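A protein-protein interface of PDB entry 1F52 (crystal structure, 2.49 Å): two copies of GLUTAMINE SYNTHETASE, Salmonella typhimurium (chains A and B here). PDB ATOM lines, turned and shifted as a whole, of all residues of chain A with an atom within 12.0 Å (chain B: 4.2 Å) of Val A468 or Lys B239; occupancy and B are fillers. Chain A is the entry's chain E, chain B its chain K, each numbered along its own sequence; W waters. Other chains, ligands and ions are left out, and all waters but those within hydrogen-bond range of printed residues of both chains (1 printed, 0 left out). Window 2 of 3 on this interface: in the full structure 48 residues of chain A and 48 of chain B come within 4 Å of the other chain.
NZ of Lys B239 lies within salt-bridge range of OXT of Val A468, 2.9 Å away.
Printed residues of chain A that touch a printed residue of chain B: Val A468.
Of the 12 printed residues of chain B, 4 touch a printed residue of chain A.
Printed residues of chain B that touch a printed residue of chain A: Lys B239, His B243, Phe B255 and Ala B364.
Hydrophobic or aromatic side chains of chain B within 4 Å of the printed part of chain A: His B243, Phe B255 and Ala B364.
NZ of Lys B239 is in hydrogen-bond range of O of Pro B363 (2.7 Å).
The backbone carbonyl oxygen of Lys B239 lies within hydrogen-bond range of a ring nitrogen (ND1) of His B243 (3.3 Å).
No position is printed for both chains.
Pro A459 touches none of the printed residues of chain B.
Leu A464 touches none of the printed residues of chain B.
No residue of chain A comes within 4 Å of Ile B235.
No residue of chain A comes within 4 Å of Gln B236.
No residue of chain A comes within 4 Å of Tyr B238.
Lys B239 touches just one residue of chain A: Val A468.
No residue of chain A comes within 4 Å of Pro B363.
Ala B364 touches just one residue of chain A: Val A468 (3.4 Å).
The nearest residue of chain A that does not touch Lys B239 is Ser A467 (6.4 Å).
Water W1 lies within hydrogen-bond range of O of Tyr A466 (2.6 Å), O of Val A468 (2.7 Å), N of Phe B255 (2.8 Å) and NE2 of His B243 (3.0 Å).
Among the printed residues, pairs that only touch across the chains: Val A468 with Ala B364 (3.4 Å), Val A468 with His B243 (3.5 Å) and Val A468 with Phe B255 (3.8 Å).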
ATOM      1  N   PRO A 459      15.300 -27.585  28.984  1.00  0.00           N
ATOM      2  CA  PRO A 459      15.181 -26.467  28.048  1.00  0.00           C
ATOM      3  C   PRO A 459      15.281 -25.110  28.726  1.00  0.00           C
ATOM      4  O   PRO A 459      15.992 -24.227  28.252  1.00  0.00           O
ATOM      5  CB  PRO A 459      13.798 -26.673  27.462  1.00  0.00           C
ATOM      6  CG  PRO A 459      13.743 -28.189  27.352  1.00  0.00           C
ATOM      7  CD  PRO A 459      14.303 -28.635  28.680  1.00  0.00           C
ATOM      8  N   VAL A 460      14.634 -24.977  29.879  1.00  0.00           N
ATOM      9  CA  VAL A 460      14.633 -23.715  30.621  1.00  0.00           C
ATOM     10  C   VAL A 460      16.025 -23.315  31.105  1.00  0.00           C
ATOM     11  O   VAL A 460      16.341 -22.125  31.250  1.00  0.00           O
ATOM     12  CB  VAL A 460      13.647 -23.780  31.788  1.00  0.00           C
ATOM     13  CG1 VAL A 460      13.732 -22.543  32.628  1.00  0.00           C
ATOM     14  CG2 VAL A 460      12.246 -23.924  31.243  1.00  0.00           C
ATOM     15  N   GLU A 461      16.892 -24.303  31.281  1.00  0.00           N
ATOM     16  CA  GLU A 461      18.239 -24.009  31.725  1.00  0.00           C
ATOM     17  C   GLU A 461      18.984 -23.222  30.679  1.00  0.00           C
ATOM     18  O   GLU A 461      19.892 -22.464  31.005  1.00  0.00           O
ATOM     19  CB  GLU A 461      18.986 -25.288  32.073  1.00  0.00           C
ATOM     20  CG  GLU A 461      18.465 -25.888  33.374  1.00  0.00           C
ATOM     21  CD  GLU A 461      19.113 -27.201  33.750  1.00  0.00           C
ATOM     22  OE1 GLU A 461      19.071 -27.549  34.947  1.00  0.00           O
ATOM     23  OE2 GLU A 461      19.626 -27.905  32.860  1.00  0.00           O
ATOM     24  N   PHE A 462      18.596 -23.401  29.412  1.00  0.00           N
ATOM     25  CA  PHE A 462      19.234 -22.650  28.311  1.00  0.00           C
ATOM     26  C   PHE A 462      18.773 -21.201  28.334  1.00  0.00           C
ATOM     27  O   PHE A 462      19.564 -20.280  28.157  1.00  0.00           O
ATOM     28  CB  PHE A 462      18.913 -23.317  26.964  1.00  0.00           C
ATOM     29  CG  PHE A 462      19.632 -24.631  26.907  1.00  0.00           C
ATOM     30  CD1 PHE A 462      20.867 -24.740  26.308  1.00  0.00           C
ATOM     31  CD2 PHE A 462      19.094 -25.747  27.520  1.00  0.00           C
ATOM     32  CE1 PHE A 462      21.567 -25.941  26.326  1.00  0.00           C
ATOM     33  CE2 PHE A 462      19.790 -26.949  27.542  1.00  0.00           C
ATOM     34  CZ  PHE A 462      21.027 -27.040  26.946  1.00  0.00           C
ATOM     35  N   GLU A 463      17.484 -21.021  28.557  1.00  0.00           N
ATOM     36  CA  GLU A 463      16.919 -19.709  28.638  1.00  0.00           C
ATOM     37  C   GLU A 463      17.603 -18.948  29.758  1.00  0.00           C
ATOM     38  O   GLU A 463      18.021 -17.798  29.587  1.00  0.00           O
ATOM     39  CB  GLU A 463      15.430 -19.848  28.870  1.00  0.00           C
ATOM     40  CG  GLU A 463      14.675 -18.561  28.955  1.00  0.00           C
ATOM     41  CD  GLU A 463      13.274 -18.803  29.455  1.00  0.00           C
ATOM     42  OE1 GLU A 463      12.660 -19.830  29.089  1.00  0.00           O
ATOM     43  OE2 GLU A 463      12.765 -17.957  30.228  1.00  0.00           O
ATOM     44  N   LEU A 464      17.729 -19.609  30.896  1.00  0.00           N
ATOM     45  CA  LEU A 464      18.327 -19.052  32.111  1.00  0.00           C
ATOM     46  C   LEU A 464      19.847 -18.936  32.083  1.00  0.00           C
ATOM     47  O   LEU A 464      20.402 -17.946  32.566  1.00  0.00           O
ATOM     48  CB  LEU A 464      18.028 -19.978  33.301  1.00  0.00           C
ATOM     49  CG  LEU A 464      16.912 -19.626  34.292  1.00  0.00           C
ATOM     50  CD1 LEU A 464      15.975 -18.579  33.692  1.00  0.00           C
ATOM     51  CD2 LEU A 464      16.156 -20.874  34.702  1.00  0.00           C
ATOM     52  N   TYR A 465      20.572 -19.921  31.525  1.00  0.00           N
ATOM     53  CA  TYR A 465      22.019 -19.861  31.615  1.00  0.00           C
ATOM     54  C   TYR A 465      22.823 -19.957  30.314  1.00  0.00           C
ATOM     55  O   TYR A 465      24.053 -19.990  30.416  1.00  0.00           O
ATOM     56  CB  TYR A 465      22.458 -20.974  32.567  1.00  0.00           C
ATOM     57  CG  TYR A 465      21.564 -21.133  33.780  1.00  0.00           C
ATOM     58  CD1 TYR A 465      20.854 -22.305  33.992  1.00  0.00           C
ATOM     59  CD2 TYR A 465      21.432 -20.109  34.709  1.00  0.00           C
ATOM     60  CE1 TYR A 465      20.039 -22.458  35.096  1.00  0.00           C
ATOM     61  CE2 TYR A 465      20.619 -20.251  35.818  1.00  0.00           C
ATOM     62  CZ  TYR A 465      19.926 -21.429  36.007  1.00  0.00           C
ATOM     63  OH  TYR A 465      19.113 -21.574  37.110  1.00  0.00           O
ATOM     64  N   TYR A 466      22.247 -19.999  29.120  1.00  0.00           N
ATOM     65  CA  TYR A 466      23.099 -20.129  27.936  1.00  0.00           C
ATOM     66  C   TYR A 466      24.117 -18.969  27.798  1.00  0.00           C
ATOM     67  O   TYR A 466      25.256 -19.190  27.402  1.00  0.00           O
ATOM     68  CB  TYR A 466      22.243 -20.238  26.672  1.00  0.00           C
ATOM     69  CG  TYR A 466      23.086 -20.427  25.416  1.00  0.00           C
ATOM     70  CD1 TYR A 466      23.569 -21.687  25.083  1.00  0.00           C
ATOM     71  CD2 TYR A 466      23.403 -19.357  24.584  1.00  0.00           C
ATOM     72  CE1 TYR A 466      24.353 -21.886  23.949  1.00  0.00           C
ATOM     73  CE2 TYR A 466      24.198 -19.541  23.438  1.00  0.00           C
ATOM     74  CZ  TYR A 466      24.665 -20.811  23.132  1.00  0.00           C
ATOM     75  OH  TYR A 466      25.424 -21.013  22.005  1.00  0.00           O
ATOM     76  N   SER A 467      23.678 -17.757  28.131  1.00  0.00           N
ATOM     77  CA  SER A 467      24.507 -16.555  28.016  1.00  0.00           C
ATOM     78  C   SER A 467      25.315 -16.221  29.260  1.00  0.00           C
ATOM     79  O   SER A 467      25.795 -15.106  29.428  1.00  0.00           O
ATOM     80  CB  SER A 467      23.626 -15.367  27.669  1.00  0.00           C
ATOM     81  OG  SER A 467      23.036 -15.538  26.395  1.00  0.00           O
ATOM     82  N   VAL A 468      25.442 -17.198  30.131  1.00  0.00           N
ATOM     83  CA  VAL A 468      26.167 -17.033  31.364  1.00  0.00           C
ATOM     84  C   VAL A 468      27.631 -16.685  31.140  1.00  0.00           C
ATOM     85  O   VAL A 468      28.140 -16.810  30.024  1.00  0.00           O
ATOM     86  CB  VAL A 468      25.995 -18.315  32.178  1.00  0.00           C
ATOM     87  CG1 VAL A 468      27.323 -19.033  32.343  1.00  0.00           C
ATOM     88  CG2 VAL A 468      25.369 -17.998  33.529  1.00  0.00           C
ATOM     89  OXT VAL A 468      28.193 -15.938  32.007  1.00  0.00           O
ATOM     90  N   ILE B 235      38.580 -12.994  33.999  1.00  0.00           N
ATOM     91  CA  ILE B 235      37.558 -13.962  33.623  1.00  0.00           C
ATOM     92  C   ILE B 235      36.496 -13.276  32.788  1.00  0.00           C
ATOM     93  O   ILE B 235      36.100 -13.782  31.742  1.00  0.00           O
ATOM     94  CB  ILE B 235      36.921 -14.595  34.847  1.00  0.00           C
ATOM     95  CG1 ILE B 235      37.798 -15.745  35.336  1.00  0.00           C
ATOM     96  CG2 ILE B 235      35.523 -15.073  34.554  1.00  0.00           C
ATOM     97  CD1 ILE B 235      38.217 -16.722  34.263  1.00  0.00           C
ATOM     98  N   GLN B 236      36.061 -12.107  33.244  1.00  0.00           N
ATOM     99  CA  GLN B 236      35.061 -11.324  32.531  1.00  0.00           C
ATOM    100  C   GLN B 236      35.517 -10.977  31.110  1.00  0.00           C
ATOM    101  O   GLN B 236      34.739 -11.047  30.149  1.00  0.00           O
ATOM    102  CB  GLN B 236      34.781 -10.035  33.289  1.00  0.00           C
ATOM    103  CG  GLN B 236      34.119 -10.228  34.615  1.00  0.00           C
ATOM    104  CD  GLN B 236      32.854 -11.023  34.500  1.00  0.00           C
ATOM    105  OE1 GLN B 236      32.889 -12.189  34.144  1.00  0.00           O
ATOM    106  NE2 GLN B 236      31.733 -10.412  34.845  1.00  0.00           N
ATOM    107  N   ILE B 237      36.785 -10.596  30.991  1.00  0.00           N
ATOM    108  CA  ILE B 237      37.380 -10.241  29.705  1.00  0.00           C
ATOM    109  C   ILE B 237      37.482 -11.497  28.868  1.00  0.00           C
ATOM    110  O   ILE B 237      37.176 -11.502  27.682  1.00  0.00           O
ATOM    111  CB  ILE B 237      38.780  -9.671  29.911  1.00  0.00           C
ATOM    112  CG1 ILE B 237      38.677  -8.281  30.541  1.00  0.00           C
ATOM    113  CG2 ILE B 237      39.547  -9.628  28.599  1.00  0.00           C
ATOM    114  CD1 ILE B 237      39.986  -7.732  30.964  1.00  0.00           C
ATOM    115  N   TYR B 238      37.886 -12.544  29.517  1.00  0.00           N
ATOM    116  CA  TYR B 238      38.018 -13.833  28.877  1.00  0.00           C
ATOM    117  C   TYR B 238      36.704 -14.228  28.221  1.00  0.00           C
ATOM    118  O   TYR B 238      36.669 -14.557  27.046  1.00  0.00           O
ATOM    119  CB  TYR B 238      38.410 -14.861  29.906  1.00  0.00           C
ATOM    120  CG  TYR B 238      38.548 -16.278  29.438  1.00  0.00           C
ATOM    121  CD1 TYR B 238      37.444 -17.087  29.222  1.00  0.00           C
ATOM    122  CD2 TYR B 238      39.813 -16.829  29.271  1.00  0.00           C
ATOM    123  CE1 TYR B 238      37.590 -18.426  28.855  1.00  0.00           C
ATOM    124  CE2 TYR B 238      39.976 -18.166  28.913  1.00  0.00           C
ATOM    125  CZ  TYR B 238      38.860 -18.960  28.709  1.00  0.00           C
ATOM    126  OH  TYR B 238      39.019 -20.289  28.352  1.00  0.00           O
ATOM    127  N   LYS B 239      35.635 -14.188  29.007  1.00  0.00           N
ATOM    128  CA  LYS B 239      34.319 -14.535  28.485  1.00  0.00           C
ATOM    129  C   LYS B 239      33.933 -13.607  27.349  1.00  0.00           C
ATOM    130  O   LYS B 239      33.388 -14.024  26.325  1.00  0.00           O
ATOM    131  CB  LYS B 239      33.271 -14.434  29.579  1.00  0.00           C
ATOM    132  CG  LYS B 239      33.405 -15.470  30.682  1.00  0.00           C
ATOM    133  CD  LYS B 239      32.204 -15.366  31.597  1.00  0.00           C
ATOM    134  CE  LYS B 239      32.168 -16.493  32.591  1.00  0.00           C
ATOM    135  NZ  LYS B 239      30.808 -16.560  33.191  1.00  0.00           N
ATOM    136  N   TYR B 240      34.224 -12.334  27.532  1.00  0.00           N
ATOM    137  CA  TYR B 240      33.891 -11.351  26.527  1.00  0.00           C
ATOM    138  C   TYR B 240      34.593 -11.677  25.221  1.00  0.00           C
ATOM    139  O   TYR B 240      33.983 -11.659  24.151  1.00  0.00           O
ATOM    140  CB  TYR B 240      34.310  -9.979  27.016  1.00  0.00           C
ATOM    141  CG  TYR B 240      33.995  -8.872  26.060  1.00  0.00           C
ATOM    142  CD1 TYR B 240      32.683  -8.474  25.833  1.00  0.00           C
ATOM    143  CD2 TYR B 240      35.009  -8.220  25.366  1.00  0.00           C
ATOM    144  CE1 TYR B 240      32.394  -7.448  24.931  1.00  0.00           C
ATOM    145  CE2 TYR B 240      34.727  -7.200  24.463  1.00  0.00           C
ATOM    146  CZ  TYR B 240      33.417  -6.820  24.247  1.00  0.00           C
ATOM    147  OH  TYR B 240      33.119  -5.847  23.310  1.00  0.00           O
ATOM    148  N   VAL B 241      35.876 -11.984  25.299  1.00  0.00           N
ATOM    149  CA  VAL B 241      36.615 -12.305  24.100  1.00  0.00           C
ATOM    150  C   VAL B 241      36.067 -13.561  23.454  1.00  0.00           C
ATOM    151  O   VAL B 241      35.836 -13.598  22.250  1.00  0.00           O
ATOM    152  CB  VAL B 241      38.096 -12.483  24.392  1.00  0.00           C
ATOM    153  CG1 VAL B 241      38.817 -13.012  23.148  1.00  0.00           C
ATOM    154  CG2 VAL B 241      38.687 -11.151  24.791  1.00  0.00           C
ATOM    155  N   VAL B 242      35.848 -14.589  24.258  1.00  0.00           N
ATOM    156  CA  VAL B 242      35.319 -15.839  23.735  1.00  0.00           C
ATOM    157  C   VAL B 242      33.981 -15.619  23.033  1.00  0.00           C
ATOM    158  O   VAL B 242      33.811 -15.982  21.868  1.00  0.00           O
ATOM    159  CB  VAL B 242      35.144 -16.866  24.852  1.00  0.00           C
ATOM    160  CG1 VAL B 242      34.309 -18.015  24.363  1.00  0.00           C
ATOM    161  CG2 VAL B 242      36.502 -17.379  25.303  1.00  0.00           C
ATOM    162  N   HIS B 243      33.060 -14.952  23.718  1.00  0.00           N
ATOM    163  CA  HIS B 243      31.740 -14.696  23.159  1.00  0.00           C
ATOM    164  C   HIS B 243      31.790 -13.921  21.870  1.00  0.00           C
ATOM    165  O   HIS B 243      31.120 -14.266  20.901  1.00  0.00           O
ATOM    166  CB  HIS B 243      30.880 -13.917  24.144  1.00  0.00           C
ATOM    167  CG  HIS B 243      30.234 -14.772  25.185  1.00  0.00           C
ATOM    168  ND1 HIS B 243      30.143 -14.395  26.502  1.00  0.00           N
ATOM    169  CD2 HIS B 243      29.619 -15.974  25.092  1.00  0.00           C
ATOM    170  CE1 HIS B 243      29.496 -15.328  27.186  1.00  0.00           C
ATOM    171  NE2 HIS B 243      29.170 -16.297  26.349  1.00  0.00           N
ATOM    172  N   PHE B 255      29.107 -20.717  28.232  1.00  0.00           N
ATOM    173  CA  PHE B 255      29.842 -21.168  29.389  1.00  0.00           C
ATOM    174  C   PHE B 255      28.935 -21.968  30.306  1.00  0.00           C
ATOM    175  O   PHE B 255      29.279 -22.192  31.449  1.00  0.00           O
ATOM    176  CB  PHE B 255      30.454 -19.985  30.111  1.00  0.00           C
ATOM    177  CG  PHE B 255      31.611 -19.377  29.374  1.00  0.00           C
ATOM    178  CD1 PHE B 255      32.895 -19.841  29.576  1.00  0.00           C
ATOM    179  CD2 PHE B 255      31.415 -18.364  28.455  1.00  0.00           C
ATOM    180  CE1 PHE B 255      33.979 -19.298  28.869  1.00  0.00           C
ATOM    181  CE2 PHE B 255      32.491 -17.817  27.742  1.00  0.00           C
ATOM    182  CZ  PHE B 255      33.771 -18.285  27.949  1.00  0.00           C
ATOM    183  N   PRO B 363      32.099 -22.514  34.953  1.00  0.00           N
ATOM    184  CA  PRO B 363      32.169 -21.160  34.403  1.00  0.00           C
ATOM    185  C   PRO B 363      30.980 -20.260  34.584  1.00  0.00           C
ATOM    186  O   PRO B 363      31.058 -19.087  34.236  1.00  0.00           O
ATOM    187  CB  PRO B 363      32.452 -21.390  32.923  1.00  0.00           C
ATOM    188  CG  PRO B 363      32.956 -22.829  32.865  1.00  0.00           C
ATOM    189  CD  PRO B 363      32.118 -23.516  33.876  1.00  0.00           C
ATOM    190  N   ALA B 364      29.869 -20.788  35.079  1.00  0.00           N
ATOM    191  CA  ALA B 364      28.685 -19.953  35.283  1.00  0.00           C
ATOM    192  C   ALA B 364      28.855 -19.100  36.530  1.00  0.00           C
ATOM    193  O   ALA B 364      28.140 -18.130  36.753  1.00  0.00           O
ATOM    194  CB  ALA B 364      27.438 -20.825  35.429  1.00  0.00           C
HETATM  195  O   HOH W   1      27.681 -18.349  27.907  1.00  0.00           O
